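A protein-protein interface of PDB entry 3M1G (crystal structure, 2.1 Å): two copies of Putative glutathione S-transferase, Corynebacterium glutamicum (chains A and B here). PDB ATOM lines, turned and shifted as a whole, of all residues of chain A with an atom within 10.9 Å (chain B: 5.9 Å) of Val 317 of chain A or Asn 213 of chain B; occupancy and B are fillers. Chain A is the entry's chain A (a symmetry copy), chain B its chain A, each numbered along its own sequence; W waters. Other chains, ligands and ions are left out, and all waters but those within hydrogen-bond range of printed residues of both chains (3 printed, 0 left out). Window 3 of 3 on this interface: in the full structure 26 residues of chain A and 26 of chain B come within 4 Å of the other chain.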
ATOM      1  N   ASP A 256     -30.546 -15.551  10.769  1.00  0.00           N
ATOM      2  CA  ASP A 256     -29.375 -14.736  10.481  1.00  0.00           C
ATOM      3  C   ASP A 256     -28.610 -14.404  11.760  1.00  0.00           C
ATOM      4  O   ASP A 256     -27.350 -14.384  11.763  1.00  0.00           O
ATOM      5  CB  ASP A 256     -29.745 -13.458   9.708  1.00  0.00           C
ATOM      6  CG  ASP A 256     -30.205 -13.744   8.267  1.00  0.00           C
ATOM      7  OD1 ASP A 256     -30.074 -14.908   7.825  1.00  0.00           O
ATOM      8  OD2 ASP A 256     -30.706 -12.801   7.592  1.00  0.00           O
ATOM      9  N   ALA A 257     -29.339 -14.194  12.857  1.00  0.00           N
ATOM     10  CA  ALA A 257     -28.724 -13.827  14.136  1.00  0.00           C
ATOM     11  C   ALA A 257     -27.863 -14.933  14.771  1.00  0.00           C
ATOM     12  O   ALA A 257     -26.855 -14.632  15.425  1.00  0.00           O
ATOM     13  CB  ALA A 257     -29.798 -13.346  15.158  1.00  0.00           C
ATOM     14  N   VAL A 258     -28.261 -16.195  14.603  1.00  0.00           N
ATOM     15  CA  VAL A 258     -27.624 -17.315  15.311  1.00  0.00           C
ATOM     16  C   VAL A 258     -27.341 -18.524  14.422  1.00  0.00           C
ATOM     17  O   VAL A 258     -26.208 -18.949  14.280  1.00  0.00           O
ATOM     18  CB  VAL A 258     -28.465 -17.814  16.514  1.00  0.00           C
ATOM     19  CG1 VAL A 258     -27.844 -19.111  17.065  1.00  0.00           C
ATOM     20  CG2 VAL A 258     -28.543 -16.738  17.605  1.00  0.00           C
ATOM     21  N   LYS A 269     -28.021 -15.998   3.664  1.00  0.00           N
ATOM     22  CA  LYS A 269     -28.762 -15.362   4.745  1.00  0.00           C
ATOM     23  C   LYS A 269     -30.246 -15.360   4.306  1.00  0.00           C
ATOM     24  O   LYS A 269     -30.551 -15.382   3.109  1.00  0.00           O
ATOM     25  CB  LYS A 269     -28.295 -13.919   5.010  1.00  0.00           C
ATOM     26  CG  LYS A 269     -26.982 -13.803   5.812  1.00  0.00           C
ATOM     27  CD  LYS A 269     -26.417 -12.381   5.862  1.00  0.00           C
ATOM     28  CE  LYS A 269     -27.298 -11.461   6.741  1.00  0.00           C
ATOM     29  NZ  LYS A 269     -26.697 -10.126   6.998  1.00  0.00           N
ATOM     30  N   PHE A 295     -33.725  -9.969  20.680  1.00  0.00           N
ATOM     31  CA  PHE A 295     -32.555 -10.425  19.922  1.00  0.00           C
ATOM     32  C   PHE A 295     -31.317 -10.584  20.802  1.00  0.00           C
ATOM     33  O   PHE A 295     -30.510 -11.482  20.568  1.00  0.00           O
ATOM     34  CB  PHE A 295     -32.265  -9.498  18.752  1.00  0.00           C
ATOM     35  CG  PHE A 295     -33.248  -9.616  17.624  1.00  0.00           C
ATOM     36  CD1 PHE A 295     -33.233 -10.710  16.798  1.00  0.00           C
ATOM     37  CD2 PHE A 295     -34.169  -8.609  17.378  1.00  0.00           C
ATOM     38  CE1 PHE A 295     -34.110 -10.805  15.743  1.00  0.00           C
ATOM     39  CE2 PHE A 295     -35.044  -8.693  16.351  1.00  0.00           C
ATOM     40  CZ  PHE A 295     -35.017  -9.805  15.511  1.00  0.00           C
ATOM     41  N   THR A 296     -31.191  -9.750  21.831  1.00  0.00           N
ATOM     42  CA  THR A 296     -30.062  -9.855  22.763  1.00  0.00           C
ATOM     43  C   THR A 296     -30.088 -11.149  23.540  1.00  0.00           C
ATOM     44  O   THR A 296     -29.070 -11.811  23.644  1.00  0.00           O
ATOM     45  CB  THR A 296     -30.005  -8.657  23.722  1.00  0.00           C
ATOM     46  OG1 THR A 296     -29.851  -7.471  22.943  1.00  0.00           O
ATOM     47  CG2 THR A 296     -28.829  -8.766  24.727  1.00  0.00           C
ATOM     48  N   LYS A 299     -29.300 -14.148  21.145  1.00  0.00           N
ATOM     49  CA  LYS A 299     -27.863 -14.289  20.803  1.00  0.00           C
ATOM     50  C   LYS A 299     -27.003 -14.666  22.004  1.00  0.00           C
ATOM     51  O   LYS A 299     -26.115 -15.519  21.924  1.00  0.00           O
ATOM     52  CB  LYS A 299     -27.328 -13.004  20.166  1.00  0.00           C
ATOM     53  CG  LYS A 299     -27.923 -12.686  18.784  1.00  0.00           C
ATOM     54  CD  LYS A 299     -27.524 -11.284  18.315  1.00  0.00           C
ATOM     55  CE  LYS A 299     -26.033 -11.181  17.933  1.00  0.00           C
ATOM     56  NZ  LYS A 299     -25.645  -9.766  17.721  1.00  0.00           N
ATOM     57  N   GLN A 300     -27.268 -14.031  23.151  1.00  0.00           N
ATOM     58  CA  GLN A 300     -26.522 -14.368  24.352  1.00  0.00           C
ATOM     59  C   GLN A 300     -26.691 -15.842  24.736  1.00  0.00           C
ATOM     60  O   GLN A 300     -25.714 -16.519  25.110  1.00  0.00           O
ATOM     61  CB  GLN A 300     -26.932 -13.463  25.505  1.00  0.00           C
ATOM     62  CG  GLN A 300     -26.369 -12.064  25.313  1.00  0.00           C
ATOM     63  CD  GLN A 300     -26.719 -11.159  26.470  1.00  0.00           C
ATOM     64  OE1 GLN A 300     -27.503 -11.526  27.302  1.00  0.00           O
ATOM     65  NE2 GLN A 300     -26.135  -9.985  26.516  1.00  0.00           N
ATOM     66  N   TYR A 303     -24.750 -18.225  21.947  1.00  0.00           N
ATOM     67  CA  TYR A 303     -23.308 -17.988  21.775  1.00  0.00           C
ATOM     68  C   TYR A 303     -22.547 -18.132  23.090  1.00  0.00           C
ATOM     69  O   TYR A 303     -21.356 -18.482  23.068  1.00  0.00           O
ATOM     70  CB  TYR A 303     -23.020 -16.610  21.145  1.00  0.00           C
ATOM     71  CG  TYR A 303     -23.210 -16.555  19.648  1.00  0.00           C
ATOM     72  CD1 TYR A 303     -22.225 -17.042  18.781  1.00  0.00           C
ATOM     73  CD2 TYR A 303     -24.377 -16.038  19.078  1.00  0.00           C
ATOM     74  CE1 TYR A 303     -22.387 -16.979  17.371  1.00  0.00           C
ATOM     75  CE2 TYR A 303     -24.532 -15.969  17.670  1.00  0.00           C
ATOM     76  CZ  TYR A 303     -23.531 -16.459  16.846  1.00  0.00           C
ATOM     77  OH  TYR A 303     -23.667 -16.414  15.488  1.00  0.00           O
ATOM     78  N   ILE A 304     -23.196 -17.849  24.226  1.00  0.00           N
ATOM     79  CA  ILE A 304     -22.520 -17.964  25.535  1.00  0.00           C
ATOM     80  C   ILE A 304     -22.679 -19.365  26.131  1.00  0.00           C
ATOM     81  O   ILE A 304     -21.736 -19.960  26.580  1.00  0.00           O
ATOM     82  CB  ILE A 304     -23.024 -16.917  26.540  1.00  0.00           C
ATOM     83  CG1 ILE A 304     -22.638 -15.517  26.047  1.00  0.00           C
ATOM     84  CG2 ILE A 304     -22.431 -17.163  27.955  1.00  0.00           C
ATOM     85  CD1 ILE A 304     -23.242 -14.377  26.906  1.00  0.00           C
ATOM     86  N   ASN A 310     -18.808 -22.989  20.774  1.00  0.00           N
ATOM     87  CA  ASN A 310     -18.206 -21.647  20.839  1.00  0.00           C
ATOM     88  C   ASN A 310     -17.473 -21.414  22.167  1.00  0.00           C
ATOM     89  O   ASN A 310     -17.947 -20.660  23.008  1.00  0.00           O
ATOM     90  CB  ASN A 310     -19.320 -20.595  20.675  1.00  0.00           C
ATOM     91  CG  ASN A 310     -18.786 -19.154  20.519  1.00  0.00           C
ATOM     92  OD1 ASN A 310     -17.776 -18.917  19.832  1.00  0.00           O
ATOM     93  ND2 ASN A 310     -19.480 -18.184  21.144  1.00  0.00           N
ATOM     94  N   ARG A 313     -17.031 -18.100  24.012  1.00  0.00           N
ATOM     95  CA  ARG A 313     -18.255 -17.473  24.515  1.00  0.00           C
ATOM     96  C   ARG A 313     -18.486 -16.008  24.099  1.00  0.00           C
ATOM     97  O   ARG A 313     -19.266 -15.287  24.733  1.00  0.00           O
ATOM     98  CB  ARG A 313     -18.346 -17.602  26.047  1.00  0.00           C
ATOM     99  CG  ARG A 313     -18.310 -19.029  26.527  1.00  0.00           C
ATOM    100  CD  ARG A 313     -18.782 -19.136  27.992  1.00  0.00           C
ATOM    101  NE  ARG A 313     -17.752 -19.777  28.740  1.00  0.00           N
ATOM    102  CZ  ARG A 313     -17.814 -20.952  29.366  1.00  0.00           C
ATOM    103  NH1 ARG A 313     -18.925 -21.682  29.400  1.00  0.00           N
ATOM    104  NH2 ARG A 313     -16.712 -21.382  29.996  1.00  0.00           N
ATOM    105  N   ILE A 314     -17.889 -15.595  22.986  1.00  0.00           N
ATOM    106  CA  ILE A 314     -18.066 -14.248  22.481  1.00  0.00           C
ATOM    107  C   ILE A 314     -19.341 -14.212  21.661  1.00  0.00           C
ATOM    108  O   ILE A 314     -19.660 -15.174  20.954  1.00  0.00           O
ATOM    109  CB  ILE A 314     -16.827 -13.835  21.709  1.00  0.00           C
ATOM    110  CG1 ILE A 314     -15.709 -13.610  22.729  1.00  0.00           C
ATOM    111  CG2 ILE A 314     -17.047 -12.558  20.853  1.00  0.00           C
ATOM    112  CD1 ILE A 314     -14.414 -13.429  22.119  1.00  0.00           C
ATOM    113  N   VAL A 315     -20.096 -13.129  21.807  1.00  0.00           N
ATOM    114  CA  VAL A 315     -21.304 -12.897  21.032  1.00  0.00           C
ATOM    115  C   VAL A 315     -20.990 -11.904  19.906  1.00  0.00           C
ATOM    116  O   VAL A 315     -20.556 -10.792  20.178  1.00  0.00           O
ATOM    117  CB  VAL A 315     -22.439 -12.313  21.921  1.00  0.00           C
ATOM    118  CG1 VAL A 315     -23.782 -12.209  21.134  1.00  0.00           C
ATOM    119  CG2 VAL A 315     -22.648 -13.170  23.204  1.00  0.00           C
ATOM    120  N   PRO A 316     -21.176 -12.302  18.638  1.00  0.00           N
ATOM    121  CA  PRO A 316     -20.898 -11.355  17.563  1.00  0.00           C
ATOM    122  C   PRO A 316     -21.749 -10.094  17.681  1.00  0.00           C
ATOM    123  O   PRO A 316     -22.913 -10.171  18.090  1.00  0.00           O
ATOM    124  CB  PRO A 316     -21.297 -12.127  16.282  1.00  0.00           C
ATOM    125  CG  PRO A 316     -21.387 -13.560  16.672  1.00  0.00           C
ATOM    126  CD  PRO A 316     -21.735 -13.565  18.137  1.00  0.00           C
ATOM    127  N   VAL A 317     -21.198  -8.958  17.290  1.00  0.00           N
ATOM    128  CA  VAL A 317     -21.971  -7.711  17.267  1.00  0.00           C
ATOM    129  C   VAL A 317     -23.060  -7.805  16.193  1.00  0.00           C
ATOM    130  O   VAL A 317     -24.171  -7.362  16.412  1.00  0.00           O
ATOM    131  CB  VAL A 317     -21.088  -6.463  17.039  1.00  0.00           C
ATOM    132  CG1 VAL A 317     -21.970  -5.158  17.062  1.00  0.00           C
ATOM    133  CG2 VAL A 317     -20.034  -6.402  18.138  1.00  0.00           C
ATOM    134  N   GLY A 318     -22.744  -8.445  15.066  1.00  0.00           N
ATOM    135  CA  GLY A 318     -23.697  -8.573  13.990  1.00  0.00           C
ATOM    136  C   GLY A 318     -24.660  -9.725  14.140  1.00  0.00           C
ATOM    137  O   GLY A 318     -24.601 -10.487  15.106  1.00  0.00           O
ATOM    138  N   PRO A 319     -25.549  -9.889  13.158  1.00  0.00           N
ATOM    139  CA  PRO A 319     -25.730  -9.074  11.986  1.00  0.00           C
ATOM    140  C   PRO A 319     -26.447  -7.755  12.275  1.00  0.00           C
ATOM    141  O   PRO A 319     -27.078  -7.587  13.325  1.00  0.00           O
ATOM    142  CB  PRO A 319     -26.626  -9.939  11.089  1.00  0.00           C
ATOM    143  CG  PRO A 319     -27.468 -10.679  12.085  1.00  0.00           C
ATOM    144  CD  PRO A 319     -26.515 -11.006  13.208  1.00  0.00           C
ATOM    145  N   ASP A 320     -26.385  -6.850  11.316  1.00  0.00           N
ATOM    146  CA  ASP A 320     -27.243  -5.678  11.352  1.00  0.00           C
ATOM    147  C   ASP A 320     -28.710  -6.123  11.209  1.00  0.00           C
ATOM    148  O   ASP A 320     -29.086  -6.775  10.233  1.00  0.00           O
ATOM    149  CB  ASP A 320     -26.862  -4.724  10.247  1.00  0.00           C
ATOM    150  CG  ASP A 320     -27.874  -3.582  10.060  1.00  0.00           C
ATOM    151  OD1 ASP A 320     -28.518  -3.170  11.017  1.00  0.00           O
ATOM    152  OD2 ASP A 320     -28.008  -3.116   8.909  1.00  0.00           O
ATOM    153  N   LEU A 321     -29.527  -5.772  12.182  1.00  0.00           N
ATOM    154  CA  LEU A 321     -30.935  -6.228  12.214  1.00  0.00           C
ATOM    155  C   LEU A 321     -31.931  -5.178  11.715  1.00  0.00           C
ATOM    156  O   LEU A 321     -33.173  -5.414  11.711  1.00  0.00           O
ATOM    157  CB  LEU A 321     -31.285  -6.610  13.663  1.00  0.00           C
ATOM    158  CG  LEU A 321     -30.517  -7.762  14.308  1.00  0.00           C
ATOM    159  CD1 LEU A 321     -30.760  -7.797  15.843  1.00  0.00           C
ATOM    160  CD2 LEU A 321     -30.844  -9.089  13.627  1.00  0.00           C
ATOM    161  N   SER A 322     -31.423  -4.032  11.278  1.00  0.00           N
ATOM    162  CA  SER A 322     -32.272  -2.900  11.006  1.00  0.00           C
ATOM    163  C   SER A 322     -33.263  -3.200   9.869  1.00  0.00           C
ATOM    164  O   SER A 322     -34.335  -2.618   9.817  1.00  0.00           O
ATOM    165  CB  SER A 322     -31.435  -1.635  10.736  1.00  0.00           C
ATOM    166  OG  SER A 322     -30.745  -1.777   9.511  1.00  0.00           O
ATOM    167  N   GLU A 358     -34.398  -3.381  20.122  1.00  0.00           N
ATOM    168  CA  GLU A 358     -33.625  -2.685  19.098  1.00  0.00           C
ATOM    169  C   GLU A 358     -34.217  -1.301  18.884  1.00  0.00           C
ATOM    170  O   GLU A 358     -35.329  -1.047  19.360  1.00  0.00           O
ATOM    171  CB  GLU A 358     -33.656  -3.469  17.785  1.00  0.00           C
ATOM    172  CG  GLU A 358     -32.934  -4.805  17.851  1.00  0.00           C
ATOM    173  CD  GLU A 358     -31.409  -4.638  18.075  1.00  0.00           C
ATOM    174  OE1 GLU A 358     -30.789  -3.744  17.463  1.00  0.00           O
ATOM    175  OE2 GLU A 358     -30.831  -5.405  18.867  1.00  0.00           O
ATOM    176  N   PRO A 359     -33.476  -0.377  18.189  1.00  0.00           N
ATOM    177  CA  PRO A 359     -34.044   0.988  18.056  1.00  0.00           C
ATOM    178  C   PRO A 359     -35.388   0.966  17.316  1.00  0.00           C
ATOM    179  O   PRO A 359     -36.198   1.816  17.525  1.00  0.00           O
ATOM    180  CB  PRO A 359     -32.966   1.781  17.278  1.00  0.00           C
ATOM    181  CG  PRO A 359     -31.660   1.009  17.481  1.00  0.00           C
ATOM    182  CD  PRO A 359     -32.084  -0.466  17.700  1.00  0.00           C
ATOM    183  N   PHE A 360     -35.641  -0.043  16.486  1.00  0.00           N
ATOM    184  CA  PHE A 360     -36.896  -0.103  15.730  1.00  0.00           C
ATOM    185  C   PHE A 360     -38.043  -0.842  16.467  1.00  0.00           C
ATOM    186  O   PHE A 360     -39.150  -0.930  15.948  1.00  0.00           O
ATOM    187  CB  PHE A 360     -36.623  -0.726  14.334  1.00  0.00           C
ATOM    188  CG  PHE A 360     -35.955  -2.092  14.390  1.00  0.00           C
ATOM    189  CD1 PHE A 360     -36.718  -3.233  14.553  1.00  0.00           C
ATOM    190  CD2 PHE A 360     -34.563  -2.205  14.334  1.00  0.00           C
ATOM    191  CE1 PHE A 360     -36.123  -4.486  14.630  1.00  0.00           C
ATOM    192  CE2 PHE A 360     -33.954  -3.438  14.410  1.00  0.00           C
ATOM    193  CZ  PHE A 360     -34.724  -4.587  14.565  1.00  0.00           C
ATOM    194  N   SER B 208     -11.747 -11.140  24.494  1.00  0.00           N
ATOM    195  CA  SER B 208     -12.815 -10.735  25.368  1.00  0.00           C
ATOM    196  C   SER B 208     -13.913 -10.128  24.491  1.00  0.00           C
ATOM    197  O   SER B 208     -13.673  -9.805  23.319  1.00  0.00           O
ATOM    198  CB  SER B 208     -12.335  -9.685  26.377  1.00  0.00           C
ATOM    199  OG  SER B 208     -11.992  -8.491  25.682  1.00  0.00           O
ATOM    200  N   GLN B 209     -15.092  -9.949  25.071  1.00  0.00           N
ATOM    201  CA  GLN B 209     -16.233  -9.391  24.345  1.00  0.00           C
ATOM    202  C   GLN B 209     -15.918  -7.968  23.928  1.00  0.00           C
ATOM    203  O   GLN B 209     -16.252  -7.531  22.822  1.00  0.00           O
ATOM    204  CB  GLN B 209     -17.482  -9.362  25.229  1.00  0.00           C
ATOM    205  CG  GLN B 209     -18.780  -8.895  24.489  1.00  0.00           C
ATOM    206  CD  GLN B 209     -19.128  -9.842  23.359  1.00  0.00           C
ATOM    207  OE1 GLN B 209     -19.262 -11.054  23.570  1.00  0.00           O
ATOM    208  NE2 GLN B 209     -19.208  -9.319  22.157  1.00  0.00           N
ATOM    209  N   GLU B 210     -15.258  -7.259  24.838  1.00  0.00           N
ATOM    210  CA  GLU B 210     -14.911  -5.854  24.661  1.00  0.00           C
ATOM    211  C   GLU B 210     -13.959  -5.698  23.490  1.00  0.00           C
ATOM    212  O   GLU B 210     -14.091  -4.778  22.703  1.00  0.00           O
ATOM    213  CB  GLU B 210     -14.250  -5.299  25.935  1.00  0.00           C
ATOM    214  CG  GLU B 210     -15.199  -5.191  27.137  1.00  0.00           C
ATOM    215  CD  GLU B 210     -15.730  -6.548  27.726  1.00  0.00           C
ATOM    216  OE1 GLU B 210     -15.051  -7.614  27.626  1.00  0.00           O
ATOM    217  OE2 GLU B 210     -16.851  -6.519  28.314  1.00  0.00           O
ATOM    218  N   ALA B 211     -13.000  -6.604  23.395  1.00  0.00           N
ATOM    219  CA  ALA B 211     -12.013  -6.565  22.332  1.00  0.00           C
ATOM    220  C   ALA B 211     -12.701  -6.888  21.014  1.00  0.00           C
ATOM    221  O   ALA B 211     -12.391  -6.291  19.999  1.00  0.00           O
ATOM    222  CB  ALA B 211     -10.843  -7.550  22.608  1.00  0.00           C
ATOM    223  N   HIS B 212     -13.638  -7.841  21.023  1.00  0.00           N
ATOM    224  CA  HIS B 212     -14.426  -8.138  19.810  1.00  0.00           C
ATOM    225  C   HIS B 212     -15.180  -6.902  19.349  1.00  0.00           C
ATOM    226  O   HIS B 212     -15.108  -6.541  18.170  1.00  0.00           O
ATOM    227  CB  HIS B 212     -15.378  -9.331  19.991  1.00  0.00           C
ATOM    228  CG  HIS B 212     -16.396  -9.454  18.895  1.00  0.00           C
ATOM    229  ND1 HIS B 212     -16.132 -10.090  17.702  1.00  0.00           N
ATOM    230  CD2 HIS B 212     -17.652  -8.961  18.790  1.00  0.00           C
ATOM    231  CE1 HIS B 212     -17.207 -10.026  16.928  1.00  0.00           C
ATOM    232  NE2 HIS B 212     -18.152  -9.364  17.578  1.00  0.00           N
ATOM    233  N   ASN B 213     -15.897  -6.278  20.265  1.00  0.00           N
ATOM    234  CA  ASN B 213     -16.732  -5.118  19.955  1.00  0.00           C
ATOM    235  C   ASN B 213     -15.951  -3.993  19.255  1.00  0.00           C
ATOM    236  O   ASN B 213     -16.417  -3.394  18.281  1.00  0.00           O
ATOM    237  CB  ASN B 213     -17.373  -4.537  21.200  1.00  0.00           C
ATOM    238  CG  ASN B 213     -18.404  -5.469  21.858  1.00  0.00           C
ATOM    239  OD1 ASN B 213     -18.825  -6.490  21.303  1.00  0.00           O
ATOM    240  ND2 ASN B 213     -18.813  -5.094  23.064  1.00  0.00           N
ATOM    241  N   GLU B 214     -14.769  -3.701  19.769  1.00  0.00           N
ATOM    242  CA  GLU B 214     -13.962  -2.619  19.218  1.00  0.00           C
ATOM    243  C   GLU B 214     -13.382  -2.978  17.857  1.00  0.00           C
ATOM    244  O   GLU B 214     -13.382  -2.166  16.952  1.00  0.00           O
ATOM    245  CB  GLU B 214     -12.836  -2.213  20.194  1.00  0.00           C
ATOM    246  CG  GLU B 214     -12.098  -0.918  19.738  1.00  0.00           C
ATOM    247  CD  GLU B 214     -13.125   0.170  19.301  1.00  0.00           C
ATOM    248  OE1 GLU B 214     -14.098   0.469  20.102  1.00  0.00           O
ATOM    249  OE2 GLU B 214     -13.000   0.651  18.127  1.00  0.00           O
ATOM    250  N   ALA B 215     -12.869  -4.184  17.719  1.00  0.00           N
ATOM    251  CA  ALA B 215     -12.307  -4.610  16.483  1.00  0.00           C
ATOM    252  C   ALA B 215     -13.376  -4.640  15.383  1.00  0.00           C
ATOM    253  O   ALA B 215     -13.131  -4.219  14.253  1.00  0.00           O
ATOM    254  CB  ALA B 215     -11.649  -5.970  16.657  1.00  0.00           C
ATOM    255  N   TYR B 216     -14.577  -5.103  15.734  1.00  0.00           N
ATOM    256  CA  TYR B 216     -15.678  -5.156  14.784  1.00  0.00           C
ATOM    257  C   TYR B 216     -16.058  -3.766  14.283  1.00  0.00           C
ATOM    258  O   TYR B 216     -16.296  -3.567  13.075  1.00  0.00           O
ATOM    259  CB  TYR B 216     -16.873  -5.868  15.435  1.00  0.00           C
ATOM    260  CG  TYR B 216     -18.186  -5.831  14.731  1.00  0.00           C
ATOM    261  CD1 TYR B 216     -18.991  -4.723  14.815  1.00  0.00           C
ATOM    262  CD2 TYR B 216     -18.654  -6.939  14.029  1.00  0.00           C
ATOM    263  CE1 TYR B 216     -20.247  -4.688  14.228  1.00  0.00           C
ATOM    264  CE2 TYR B 216     -19.904  -6.917  13.403  1.00  0.00           C
ATOM    265  CZ  TYR B 216     -20.685  -5.787  13.522  1.00  0.00           C
ATOM    266  OH  TYR B 216     -21.912  -5.737  12.960  1.00  0.00           O
ATOM    267  N   LYS B 217     -16.135  -2.824  15.210  1.00  0.00           N
ATOM    268  CA  LYS B 217     -16.481  -1.474  14.872  1.00  0.00           C
ATOM    269  C   LYS B 217     -15.458  -0.912  13.896  1.00  0.00           C
ATOM    270  O   LYS B 217     -15.832  -0.354  12.888  1.00  0.00           O
ATOM    271  CB  LYS B 217     -16.516  -0.606  16.125  1.00  0.00           C
ATOM    272  CG  LYS B 217     -17.201   0.733  15.947  1.00  0.00           C
ATOM    273  CD  LYS B 217     -16.946   1.611  17.190  1.00  0.00           C
ATOM    274  CE  LYS B 217     -17.757   2.897  17.186  1.00  0.00           C
ATOM    275  NZ  LYS B 217     -17.215   3.874  18.236  1.00  0.00           N
ATOM    276  N   ARG B 218     -14.178  -1.090  14.191  1.00  0.00           N
ATOM    277  CA  ARG B 218     -13.117  -0.625  13.286  1.00  0.00           C
ATOM    278  C   ARG B 218     -13.215  -1.245  11.900  1.00  0.00           C
ATOM    279  O   ARG B 218     -13.076  -0.557  10.888  1.00  0.00           O
ATOM    280  CB  ARG B 218     -11.727  -0.872  13.893  1.00  0.00           C
ATOM    281  CG  ARG B 218     -11.356   0.163  14.977  1.00  0.00           C
ATOM    282  CD  ARG B 218     -10.051  -0.209  15.685  1.00  0.00           C
ATOM    283  NE  ARG B 218      -8.881  -0.209  14.779  1.00  0.00           N
ATOM    284  CZ  ARG B 218      -7.647  -0.545  15.158  1.00  0.00           C
ATOM    285  NH1 ARG B 218      -7.415  -0.957  16.396  1.00  0.00           N
ATOM    286  NH2 ARG B 218      -6.652  -0.506  14.306  1.00  0.00           N
ATOM    287  N   LYS B 264     -16.533 -14.110  13.235  1.00  0.00           N
ATOM    288  CA  LYS B 264     -17.656 -13.309  13.757  1.00  0.00           C
ATOM    289  C   LYS B 264     -17.672 -11.888  13.210  1.00  0.00           C
ATOM    290  O   LYS B 264     -18.144 -10.979  13.873  1.00  0.00           O
ATOM    291  CB  LYS B 264     -17.624 -13.298  15.288  1.00  0.00           C
ATOM    292  CG  LYS B 264     -17.657 -14.714  15.935  1.00  0.00           C
ATOM    293  CD  LYS B 264     -17.842 -14.641  17.451  1.00  0.00           C
ATOM    294  CE  LYS B 264     -18.075 -16.023  18.083  1.00  0.00           C
ATOM    295  NZ  LYS B 264     -16.878 -16.920  18.056  1.00  0.00           N
HETATM  296  O   HOH W   1     -20.921 -10.191  13.576  1.00  0.00           O
HETATM  297  O   HOH W   2     -22.430  -8.895  20.914  1.00  0.00           O
HETATM  298  O   HOH W   3     -19.744 -12.542  25.726  1.00  0.00           O
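The backbone carbonyl oxygen of Val 315 of chain A lies within hydrogen-bond range of the side-chain amide nitrogen of Gln 209 of chain B (2.8 Å).
The side-chain amino group (NZ) of Lys 264 of chain B is in hydrogen-bond range of the side-chain amide oxygen (OD1) of Asn 310 of chain A (2.8 Å).
NE2 of His 212 of chain B lies within hydrogen-bond range of N of Val 317 of chain A (3.1 Å).
NZ of Lys 299 of chain A sits at hydrogen-bond distance from O of Gly 318 of chain A, at 2.9 Å.
The backbone carbonyl oxygen of Tyr 303 of chain A is in hydrogen-bond range of the side-chain amide nitrogen of Asn 310 of chain A, at 2.7 Å.
NZ of Lys 299 of chain A lies within hydrogen-bond range of O of Val 317 of chain A, at 3.1 Å.
The side-chain amide nitrogen of Gln 209 of chain B is in hydrogen-bond range of the side-chain amide oxygen of Asn 213 of chain B, 3.0 Å away.
The backbone carbonyl oxygen of Ile 314 of chain A is in hydrogen-bond range of the side-chain amide nitrogen of Asn 310 of chain A (3.0 Å).
O of Pro 316 of chain A sits at hydrogen-bond distance from NZ of Lys 299 of chain A, at 2.8 Å.
Ile 314 of chain A touches Ser 208 of chain B.
CA of Ile 314 of chain A touches OE1 of Gln 209 of chain B, 3.6 Å away.
His 212 of chain B touches Ile 314 of chain A (CG to CG2, 3.7 Å).
Ile 314 of chain A touches Lys 264 of chain B (O to CE, 3.4 Å).
O of Val 315 of chain A touches CD2 of His 212 of chain B, at 3.7 Å.
NE2 of His 212 of chain B touches CA of Pro 316 of chain A (3.4 Å).
Pro 316 of chain A touches Lys 264 of chain B.
Val 317 of chain A touches Asn 213 of chain B.
Tyr 216 of chain B touches Val 317 of chain A.
Gly 318 of chain A touches Tyr 216 of chain B (CA to OH, 3.5 Å).
Val 317 of chain A touches just these residues of chain B: His 212, Asn 213 and Tyr 216.
Asn 213 of chain B touches one residue of chain A.
Of chain A, only Ile 314 and Val 315 come within 4 Å of Gln 209 of chain B.
No residue of chain A comes within 4 Å of Glu 214 of chain B.
Ala 215 of chain B touches none of the printed residues of chain A.
Of chain A, only Val 317 (3.3 Å) and Gly 318 (3.5 Å) come within 4 Å of Tyr 216 of chain B.
Of the printed residues of chain B, Asn 310 of chain A touches Lys 264 (2.8 Å).
Of the printed residues of chain B, Val 315 of chain A touches Gln 209 and His 212.
The nearest printed residue of chain B that does not touch Val 317 of chain A is Lys 264 of chain B (5.0 Å).
Of the 12 printed residues of chain B, 6 touch a printed residue of chain A.
Hydrophobic or aromatic side chains of chain B that line the printed part of chain A: His 212 and Tyr 216.
Of the 24 printed residues of chain A, 6 touch a printed residue of chain B.
Hydrophobic or aromatic side chains of chain A that line the printed part of chain B: Ile 314, Val 315, Pro 316 and Val 317.
Among the printed residues, no Asp or Glu carboxylate lies within 4 Å of a Lys or Arg side-chain nitrogen of the other chain.
No position is printed for both chains.
Water W3 lies within hydrogen-bond range of the side-chain amide oxygen of Gln 209 of chain B (2.7 Å) and the backbone carbonyl oxygen of Arg 313 of chain A (3.0 Å).
Water W2 lies within hydrogen-bond range of O of Val 315 of chain A (2.8 Å), O of Pro 316 of chain A (3.1 Å) and NE2 of Gln 209 of chain B (3.5 Å).
Water W1 bridges O of Lys 264 of chain B and N of Gly 318 of chain A.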
